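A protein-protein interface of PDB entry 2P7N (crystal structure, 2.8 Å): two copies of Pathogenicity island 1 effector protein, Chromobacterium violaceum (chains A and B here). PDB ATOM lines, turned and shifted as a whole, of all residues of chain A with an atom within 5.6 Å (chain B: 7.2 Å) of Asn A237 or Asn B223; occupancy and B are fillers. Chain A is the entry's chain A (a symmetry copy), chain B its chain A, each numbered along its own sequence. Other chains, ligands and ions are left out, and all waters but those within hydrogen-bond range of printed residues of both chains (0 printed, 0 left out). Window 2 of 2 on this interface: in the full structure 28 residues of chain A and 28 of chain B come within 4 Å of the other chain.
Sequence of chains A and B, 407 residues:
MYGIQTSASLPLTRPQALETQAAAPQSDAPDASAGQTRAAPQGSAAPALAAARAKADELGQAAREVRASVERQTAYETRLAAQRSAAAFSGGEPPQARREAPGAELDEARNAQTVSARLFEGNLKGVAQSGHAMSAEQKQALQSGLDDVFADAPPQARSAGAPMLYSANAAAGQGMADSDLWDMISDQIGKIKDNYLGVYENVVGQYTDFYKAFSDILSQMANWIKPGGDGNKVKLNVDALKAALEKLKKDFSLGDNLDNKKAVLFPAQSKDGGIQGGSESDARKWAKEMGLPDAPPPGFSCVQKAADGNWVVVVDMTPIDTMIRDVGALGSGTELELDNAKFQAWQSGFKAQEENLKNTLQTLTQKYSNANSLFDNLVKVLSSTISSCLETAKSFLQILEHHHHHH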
ATOM      1  N   TRP A 224      -1.495  18.140 -29.443  1.00  0.00           N
ATOM      2  CA  TRP A 224      -0.674  18.929 -28.533  1.00  0.00           C
ATOM      3  C   TRP A 224      -1.507  19.501 -27.388  1.00  0.00           C
ATOM      4  O   TRP A 224      -1.019  20.318 -26.601  1.00  0.00           O
ATOM      5  CB  TRP A 224       0.029  20.067 -29.280  1.00  0.00           C
ATOM      6  CG  TRP A 224       0.908  19.600 -30.404  1.00  0.00           C
ATOM      7  CD1 TRP A 224       1.705  18.493 -30.418  1.00  0.00           C
ATOM      8  CD2 TRP A 224       1.066  20.227 -31.681  1.00  0.00           C
ATOM      9  NE1 TRP A 224       2.355  18.394 -31.623  1.00  0.00           N
ATOM     10  CE2 TRP A 224       1.994  19.455 -32.415  1.00  0.00           C
ATOM     11  CE3 TRP A 224       0.547  21.390 -32.267  1.00  0.00           C
ATOM     12  CZ2 TRP A 224       2.371  19.773 -33.724  1.00  0.00           C
ATOM     13  CZ3 TRP A 224       0.919  21.711 -33.566  1.00  0.00           C
ATOM     14  CH2 TRP A 224       1.839  20.911 -34.276  1.00  0.00           C
ATOM     15  N   ILE A 225      -2.760  19.065 -27.299  1.00  0.00           N
ATOM     16  CA  ILE A 225      -3.659  19.522 -26.251  1.00  0.00           C
ATOM     17  C   ILE A 225      -4.936  18.698 -26.211  1.00  0.00           C
ATOM     18  O   ILE A 225      -4.904  17.507 -25.907  1.00  0.00           O
ATOM     19  CB  ILE A 225      -4.034  21.010 -26.437  1.00  0.00           C
ATOM     20  CG1 ILE A 225      -5.134  21.385 -25.445  1.00  0.00           C
ATOM     21  CG2 ILE A 225      -4.479  21.272 -27.859  1.00  0.00           C
ATOM     22  CD1 ILE A 225      -5.510  22.839 -25.478  1.00  0.00           C
ATOM     23  N   LYS A 235      -1.168  19.186 -20.345  1.00  0.00           N
ATOM     24  CA  LYS A 235      -2.240  19.972 -20.925  1.00  0.00           C
ATOM     25  C   LYS A 235      -1.767  20.650 -22.198  1.00  0.00           C
ATOM     26  O   LYS A 235      -2.436  20.571 -23.226  1.00  0.00           O
ATOM     27  CB  LYS A 235      -2.706  21.041 -19.931  1.00  0.00           C
ATOM     28  CG  LYS A 235      -4.196  21.298 -19.969  1.00  0.00           C
ATOM     29  CD  LYS A 235      -4.744  21.456 -18.557  1.00  0.00           C
ATOM     30  CE  LYS A 235      -6.013  20.636 -18.369  1.00  0.00           C
ATOM     31  NZ  LYS A 235      -6.097  20.041 -17.004  1.00  0.00           N
ATOM     32  N   LEU A 236      -0.610  21.294 -22.137  1.00  0.00           N
ATOM     33  CA  LEU A 236      -0.108  22.011 -23.293  1.00  0.00           C
ATOM     34  C   LEU A 236       1.265  21.606 -23.767  1.00  0.00           C
ATOM     35  O   LEU A 236       2.159  21.333 -22.959  1.00  0.00           O
ATOM     36  CB  LEU A 236      -0.055  23.519 -22.973  1.00  0.00           C
ATOM     37  CG  LEU A 236      -0.496  24.487 -24.073  1.00  0.00           C
ATOM     38  CD1 LEU A 236      -1.170  23.721 -25.204  1.00  0.00           C
ATOM     39  CD2 LEU A 236      -1.435  25.513 -23.500  1.00  0.00           C
ATOM     40  N   ASN A 237       1.408  21.511 -25.081  1.00  0.00           N
ATOM     41  CA  ASN A 237       2.733  21.325 -25.652  1.00  0.00           C
ATOM     42  C   ASN A 237       3.087  22.699 -26.286  1.00  0.00           C
ATOM     43  O   ASN A 237       3.163  22.841 -27.512  1.00  0.00           O
ATOM     44  CB  ASN A 237       2.767  20.272 -26.744  1.00  0.00           C
ATOM     45  CG  ASN A 237       4.171  19.817 -27.042  1.00  0.00           C
ATOM     46  OD1 ASN A 237       4.428  18.626 -27.144  1.00  0.00           O
ATOM     47  ND2 ASN A 237       5.088  20.761 -27.193  1.00  0.00           N
ATOM     48  N   VAL A 238       3.307  23.713 -25.447  1.00  0.00           N
ATOM     49  CA  VAL A 238       3.635  25.048 -25.929  1.00  0.00           C
ATOM     50  C   VAL A 238       4.838  25.051 -26.874  1.00  0.00           C
ATOM     51  O   VAL A 238       5.011  25.987 -27.653  1.00  0.00           O
ATOM     52  CB  VAL A 238       3.894  25.996 -24.748  1.00  0.00           C
ATOM     53  CG1 VAL A 238       4.492  27.304 -25.232  1.00  0.00           C
ATOM     54  CG2 VAL A 238       2.588  26.262 -24.011  1.00  0.00           C
ATOM     55  N   ASP A 239       5.662  24.010 -26.824  1.00  0.00           N
ATOM     56  CA  ASP A 239       6.834  23.951 -27.696  1.00  0.00           C
ATOM     57  C   ASP A 239       6.489  23.605 -29.137  1.00  0.00           C
ATOM     58  O   ASP A 239       6.789  24.370 -30.056  1.00  0.00           O
ATOM     59  CB  ASP A 239       7.853  22.937 -27.167  1.00  0.00           C
ATOM     60  CG  ASP A 239       8.952  23.588 -26.346  1.00  0.00           C
ATOM     61  OD1 ASP A 239       9.890  24.157 -26.938  1.00  0.00           O
ATOM     62  OD2 ASP A 239       8.872  23.537 -25.106  1.00  0.00           O
ATOM     63  N   ALA A 240       5.865  22.449 -29.333  1.00  0.00           N
ATOM     64  CA  ALA A 240       5.484  22.001 -30.669  1.00  0.00           C
ATOM     65  C   ALA A 240       4.526  22.984 -31.341  1.00  0.00           C
ATOM     66  O   ALA A 240       4.583  23.181 -32.550  1.00  0.00           O
ATOM     67  CB  ALA A 240       4.844  20.623 -30.588  1.00  0.00           C
ATOM     68  N   LEU A 241       3.646  23.597 -30.554  1.00  0.00           N
ATOM     69  CA  LEU A 241       2.690  24.556 -31.092  1.00  0.00           C
ATOM     70  C   LEU A 241       3.424  25.817 -31.515  1.00  0.00           C
ATOM     71  O   LEU A 241       3.197  26.343 -32.599  1.00  0.00           O
ATOM     72  CB  LEU A 241       1.628  24.899 -30.049  1.00  0.00           C
ATOM     73  CG  LEU A 241       0.476  25.815 -30.480  1.00  0.00           C
ATOM     74  CD1 LEU A 241      -0.633  25.762 -29.438  1.00  0.00           C
ATOM     75  CD2 LEU A 241       0.962  27.239 -30.657  1.00  0.00           C
ATOM     76  N   LYS A 242       4.307  26.304 -30.650  1.00  0.00           N
ATOM     77  CA  LYS A 242       5.068  27.511 -30.943  1.00  0.00           C
ATOM     78  C   LYS A 242       6.135  27.233 -32.000  1.00  0.00           C
ATOM     79  O   LYS A 242       6.609  28.154 -32.667  1.00  0.00           O
ATOM     80  CB  LYS A 242       5.733  28.046 -29.675  1.00  0.00           C
ATOM     81  CG  LYS A 242       6.264  29.459 -29.822  1.00  0.00           C
ATOM     82  CD  LYS A 242       7.188  29.839 -28.676  1.00  0.00           C
ATOM     83  CE  LYS A 242       7.838  31.192 -28.931  1.00  0.00           C
ATOM     84  NZ  LYS A 242       8.771  31.578 -27.842  1.00  0.00           N
ATOM     85  N   ALA A 243       6.510  25.966 -32.148  1.00  0.00           N
ATOM     86  CA  ALA A 243       7.514  25.577 -33.123  1.00  0.00           C
ATOM     87  C   ALA A 243       6.909  25.581 -34.524  1.00  0.00           C
ATOM     88  O   ALA A 243       7.553  25.999 -35.487  1.00  0.00           O
ATOM     89  CB  ALA A 243       8.061  24.203 -32.791  1.00  0.00           C
ATOM     90  N   GLY A 333       7.822  25.383 -22.456  1.00  0.00           N
ATOM     91  CA  GLY A 333       7.914  24.004 -22.015  1.00  0.00           C
ATOM     92  C   GLY A 333       6.940  23.067 -22.636  1.00  0.00           C
ATOM     93  O   GLY A 333       5.798  23.443 -22.833  1.00  0.00           O
ATOM     94  N   THR A 334       7.367  21.839 -22.879  1.00  0.00           N
ATOM     95  CA  THR A 334       6.525  20.874 -23.561  1.00  0.00           C
ATOM     96  C   THR A 334       5.327  20.418 -22.767  1.00  0.00           C
ATOM     97  O   THR A 334       4.630  19.488 -23.163  1.00  0.00           O
ATOM     98  CB  THR A 334       7.363  19.653 -23.986  1.00  0.00           C
ATOM     99  OG1 THR A 334       6.593  18.468 -23.830  1.00  0.00           O
ATOM    100  CG2 THR A 334       8.557  19.487 -23.071  1.00  0.00           C
ATOM    101  N   LEU A 336       3.346  21.378 -20.219  1.00  0.00           N
ATOM    102  CA  LEU A 336       2.966  22.541 -19.426  1.00  0.00           C
ATOM    103  C   LEU A 336       1.506  22.507 -19.011  1.00  0.00           C
ATOM    104  O   LEU A 336       0.609  22.727 -19.827  1.00  0.00           O
ATOM    105  CB  LEU A 336       3.263  23.822 -20.201  1.00  0.00           C
ATOM    106  CG  LEU A 336       2.461  25.090 -19.900  1.00  0.00           C
ATOM    107  CD1 LEU A 336       2.316  25.323 -18.407  1.00  0.00           C
ATOM    108  CD2 LEU A 336       3.167  26.261 -20.559  1.00  0.00           C
ATOM    109  N   ALA B  88      17.103  15.433 -32.134  1.00  0.00           N
ATOM    110  CA  ALA B  88      15.767  15.008 -31.735  1.00  0.00           C
ATOM    111  C   ALA B  88      15.805  13.885 -30.697  1.00  0.00           C
ATOM    112  O   ALA B  88      15.147  13.966 -29.660  1.00  0.00           O
ATOM    113  CB  ALA B  88      14.979  14.561 -32.958  1.00  0.00           C
ATOM    114  N   PRO B  95      17.533  21.138 -32.203  1.00  0.00           N
ATOM    115  CA  PRO B  95      17.549  21.124 -33.634  1.00  0.00           C
ATOM    116  C   PRO B  95      17.803  22.626 -33.961  1.00  0.00           C
ATOM    117  O   PRO B  95      16.843  23.431 -34.191  1.00  0.00           O
ATOM    118  CB  PRO B  95      16.106  20.809 -33.989  1.00  0.00           C
ATOM    119  CG  PRO B  95      15.731  19.810 -32.985  1.00  0.00           C
ATOM    120  CD  PRO B  95      16.443  20.256 -31.688  1.00  0.00           C
ATOM    121  N   ILE B 217      10.331  17.900 -40.270  1.00  0.00           N
ATOM    122  CA  ILE B 217       9.612  17.068 -39.327  1.00  0.00           C
ATOM    123  C   ILE B 217      10.552  16.608 -38.209  1.00  0.00           C
ATOM    124  O   ILE B 217      10.147  16.522 -37.053  1.00  0.00           O
ATOM    125  CB  ILE B 217       8.987  15.841 -40.034  1.00  0.00           C
ATOM    126  CG1 ILE B 217       7.709  16.274 -40.757  1.00  0.00           C
ATOM    127  CG2 ILE B 217       8.703  14.727 -39.027  1.00  0.00           C
ATOM    128  CD1 ILE B 217       7.034  15.182 -41.571  1.00  0.00           C
ATOM    129  N   LEU B 218      11.802  16.323 -38.560  1.00  0.00           N
ATOM    130  CA  LEU B 218      12.782  15.893 -37.580  1.00  0.00           C
ATOM    131  C   LEU B 218      12.980  16.987 -36.528  1.00  0.00           C
ATOM    132  O   LEU B 218      13.166  16.704 -35.338  1.00  0.00           O
ATOM    133  CB  LEU B 218      14.121  15.594 -38.255  1.00  0.00           C
ATOM    134  CG  LEU B 218      14.133  14.520 -39.340  1.00  0.00           C
ATOM    135  CD1 LEU B 218      15.560  14.321 -39.831  1.00  0.00           C
ATOM    136  CD2 LEU B 218      13.574  13.217 -38.790  1.00  0.00           C
ATOM    137  N   SER B 219      12.935  18.239 -36.972  1.00  0.00           N
ATOM    138  CA  SER B 219      13.103  19.375 -36.077  1.00  0.00           C
ATOM    139  C   SER B 219      11.990  19.402 -35.044  1.00  0.00           C
ATOM    140  O   SER B 219      12.238  19.624 -33.864  1.00  0.00           O
ATOM    141  CB  SER B 219      13.098  20.681 -36.874  1.00  0.00           C
ATOM    142  OG  SER B 219      14.104  20.670 -37.878  1.00  0.00           O
ATOM    143  N   GLN B 220      10.760  19.182 -35.493  1.00  0.00           N
ATOM    144  CA  GLN B 220       9.617  19.178 -34.588  1.00  0.00           C
ATOM    145  C   GLN B 220       9.560  17.878 -33.786  1.00  0.00           C
ATOM    146  O   GLN B 220       9.003  17.837 -32.688  1.00  0.00           O
ATOM    147  CB  GLN B 220       8.321  19.380 -35.376  1.00  0.00           C
ATOM    148  CG  GLN B 220       8.118  20.823 -35.835  1.00  0.00           C
ATOM    149  CD  GLN B 220       6.869  21.018 -36.683  1.00  0.00           C
ATOM    150  OE1 GLN B 220       6.874  20.765 -37.890  1.00  0.00           O
ATOM    151  NE2 GLN B 220       5.790  21.462 -36.046  1.00  0.00           N
ATOM    152  N   MET B 221      10.156  16.822 -34.333  1.00  0.00           N
ATOM    153  CA  MET B 221      10.182  15.530 -33.663  1.00  0.00           C
ATOM    154  C   MET B 221      10.892  15.672 -32.322  1.00  0.00           C
ATOM    155  O   MET B 221      10.606  14.939 -31.371  1.00  0.00           O
ATOM    156  CB  MET B 221      10.904  14.497 -34.526  1.00  0.00           C
ATOM    157  CG  MET B 221      10.841  13.075 -33.984  1.00  0.00           C
ATOM    158  SD  MET B 221      11.748  11.925 -35.032  1.00  0.00           S
ATOM    159  CE  MET B 221      11.064  12.316 -36.619  1.00  0.00           C
ATOM    160  N   ALA B 222      11.814  16.627 -32.257  1.00  0.00           N
ATOM    161  CA  ALA B 222      12.579  16.880 -31.050  1.00  0.00           C
ATOM    162  C   ALA B 222      11.663  17.103 -29.855  1.00  0.00           C
ATOM    163  O   ALA B 222      11.928  16.602 -28.762  1.00  0.00           O
ATOM    164  CB  ALA B 222      13.477  18.090 -31.247  1.00  0.00           C
ATOM    165  N   ASN B 223      10.588  17.853 -30.061  1.00  0.00           N
ATOM    166  CA  ASN B 223       9.649  18.146 -28.986  1.00  0.00           C
ATOM    167  C   ASN B 223       8.659  17.002 -28.758  1.00  0.00           C
ATOM    168  O   ASN B 223       7.767  17.104 -27.917  1.00  0.00           O
ATOM    169  CB  ASN B 223       8.868  19.426 -29.294  1.00  0.00           C
ATOM    170  CG  ASN B 223       9.649  20.396 -30.154  1.00  0.00           C
ATOM    171  OD1 ASN B 223       9.639  20.302 -31.388  1.00  0.00           O
ATOM    172  ND2 ASN B 223      10.339  21.331 -29.511  1.00  0.00           N
ATOM    173  N   TRP B 224       8.809  15.917 -29.511  1.00  0.00           N
ATOM    174  CA  TRP B 224       7.918  14.773 -29.359  1.00  0.00           C
ATOM    175  C   TRP B 224       8.633  13.596 -28.698  1.00  0.00           C
ATOM    176  O   TRP B 224       8.088  12.491 -28.622  1.00  0.00           O
ATOM    177  CB  TRP B 224       7.353  14.339 -30.715  1.00  0.00           C
ATOM    178  CG  TRP B 224       6.595  15.421 -31.429  1.00  0.00           C
ATOM    179  CD1 TRP B 224       5.763  16.346 -30.870  1.00  0.00           C
ATOM    180  CD2 TRP B 224       6.613  15.692 -32.835  1.00  0.00           C
ATOM    181  NE1 TRP B 224       5.255  17.173 -31.842  1.00  0.00           N
ATOM    182  CE2 TRP B 224       5.748  16.786 -33.062  1.00  0.00           C
ATOM    183  CE3 TRP B 224       7.243  15.094 -33.935  1.00  0.00           C
ATOM    184  CZ2 TRP B 224       5.541  17.331 -34.333  1.00  0.00           C
ATOM    185  CZ3 TRP B 224       7.040  15.630 -35.199  1.00  0.00           C
ATOM    186  CH2 TRP B 224       6.178  16.732 -35.390  1.00  0.00           C
ATOM    187  N   ILE B 225       9.848  13.843 -28.219  1.00  0.00           N
ATOM    188  CA  ILE B 225      10.635  12.814 -27.558  1.00  0.00           C
ATOM    189  C   ILE B 225      11.865  13.397 -26.881  1.00  0.00           C
ATOM    190  O   ILE B 225      11.751  14.169 -25.931  1.00  0.00           O
ATOM    191  CB  ILE B 225      11.088  11.721 -28.553  1.00  0.00           C
ATOM    192  CG1 ILE B 225      12.077  10.783 -27.863  1.00  0.00           C
ATOM    193  CG2 ILE B 225      11.707  12.346 -29.783  1.00  0.00           C
ATOM    194  CD1 ILE B 225      12.512   9.626 -28.717  1.00  0.00           C
ATOM    195  N   ASN B 237       5.547  10.721 -28.420  1.00  0.00           N
ATOM    196  CA  ASN B 237       4.293  11.265 -28.916  1.00  0.00           C
ATOM    197  C   ASN B 237       4.070  10.561 -30.284  1.00  0.00           C
ATOM    198  O   ASN B 237       4.144  11.186 -31.349  1.00  0.00           O
ATOM    199  CB  ASN B 237       4.347  12.763 -29.153  1.00  0.00           C
ATOM    200  CG  ASN B 237       2.970  13.361 -29.282  1.00  0.00           C
ATOM    201  OD1 ASN B 237       2.680  14.384 -28.679  1.00  0.00           O
ATOM    202  ND2 ASN B 237       2.115  12.732 -30.075  1.00  0.00           N
ATOM    203  N   ALA B 240       1.663  12.697 -32.873  1.00  0.00           N
ATOM    204  CA  ALA B 240       2.180  13.842 -33.617  1.00  0.00           C
ATOM    205  C   ALA B 240       3.248  13.421 -34.626  1.00  0.00           C
ATOM    206  O   ALA B 240       3.342  13.990 -35.708  1.00  0.00           O
ATOM    207  CB  ALA B 240       2.751  14.869 -32.651  1.00  0.00           C
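Trp A224 touches its own counterpart, Trp B224. Trp A224 touches Ala B240, and with the chains exchanged Ala A240 touches Trp B224. Of the 5 pairs that touch across the chains among the printed residues, 3 have their exchanged pair printed and touching as well.
Asn A237 touches one residue of chain B. Printed residues of chain A within 4 Å of Asn B223: Asn A237 and Asp A239. Printed residues of chain A within 4 Å of Ala B240: Trp A224. Of the printed residues of chain B, Ala A240 touches Trp B224. Printed residues of chain A within 4 Å of Trp B224: Trp A224 and Ala A240. Printed residues of chain B within 4 Å of Asp A239: Asn B223 (3.8 Å). Of the printed residues of chain B, Trp A224 touches Trp B224 (3.2 Å) and Ala B240 (3.7 Å). Ile B225 touches none of the printed residues of chain A. Thr A334 touches none of the printed residues of chain B. The nearest printed residue of chain B that does not touch Asp A239 is Gln B220 (6.7 Å).
The backbone carbonyl oxygen of Gln B220 sits close to the side-chain amide oxygen of Asn B223 (2.9 Å). The backbone NH (N) of Asn B237 is in hydrogen-bond range of the backbone carbonyl oxygen (O) of Trp B224 (3.1 Å). O of Trp A224 sits at hydrogen-bond distance from N of Asn A237, at 3.1 Å. The side-chain amide nitrogen (ND2) of Asn A237 lies close to the backbone NH (N) of Asp A239 (3.3 Å). The side-chain carboxylate (OD2) of Asp A239 sits close to the backbone NH (N) of Gly A333, 3.4 Å away. The backbone NH (N) of Thr A334 sits at hydrogen-bond distance from the side-chain carboxylate (OD2) of Asp A239, at 3.2 Å.
The indole nitrogen (NE1) of Trp B224 lies close to the indole nitrogen (NE1) of Trp A224 (3.2 Å).
Of the 14 printed residues of chain A, 4 touch a printed residue of chain B. Hydrophobic or aromatic side chains of chain A that line the printed part of chain B: Trp A224 and Ala A240. Of the 13 printed residues of chain B, 3 touch a printed residue of chain A. Among the printed residues, 5 pairs touch across the chains. Among the printed residues, no Asp or Glu carboxylate lies within 4 Å of a Lys or Arg side-chain nitrogen of the other chain.
Ala B240 touches Trp A224 (CB to NE1, 3.7 Å). Asn B223 touches Asn A237 (O to OD1, 3.8 Å). Asp A239 touches Asn B223 (CB to ND2, 3.8 Å). Ala A240 touches Trp B224.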
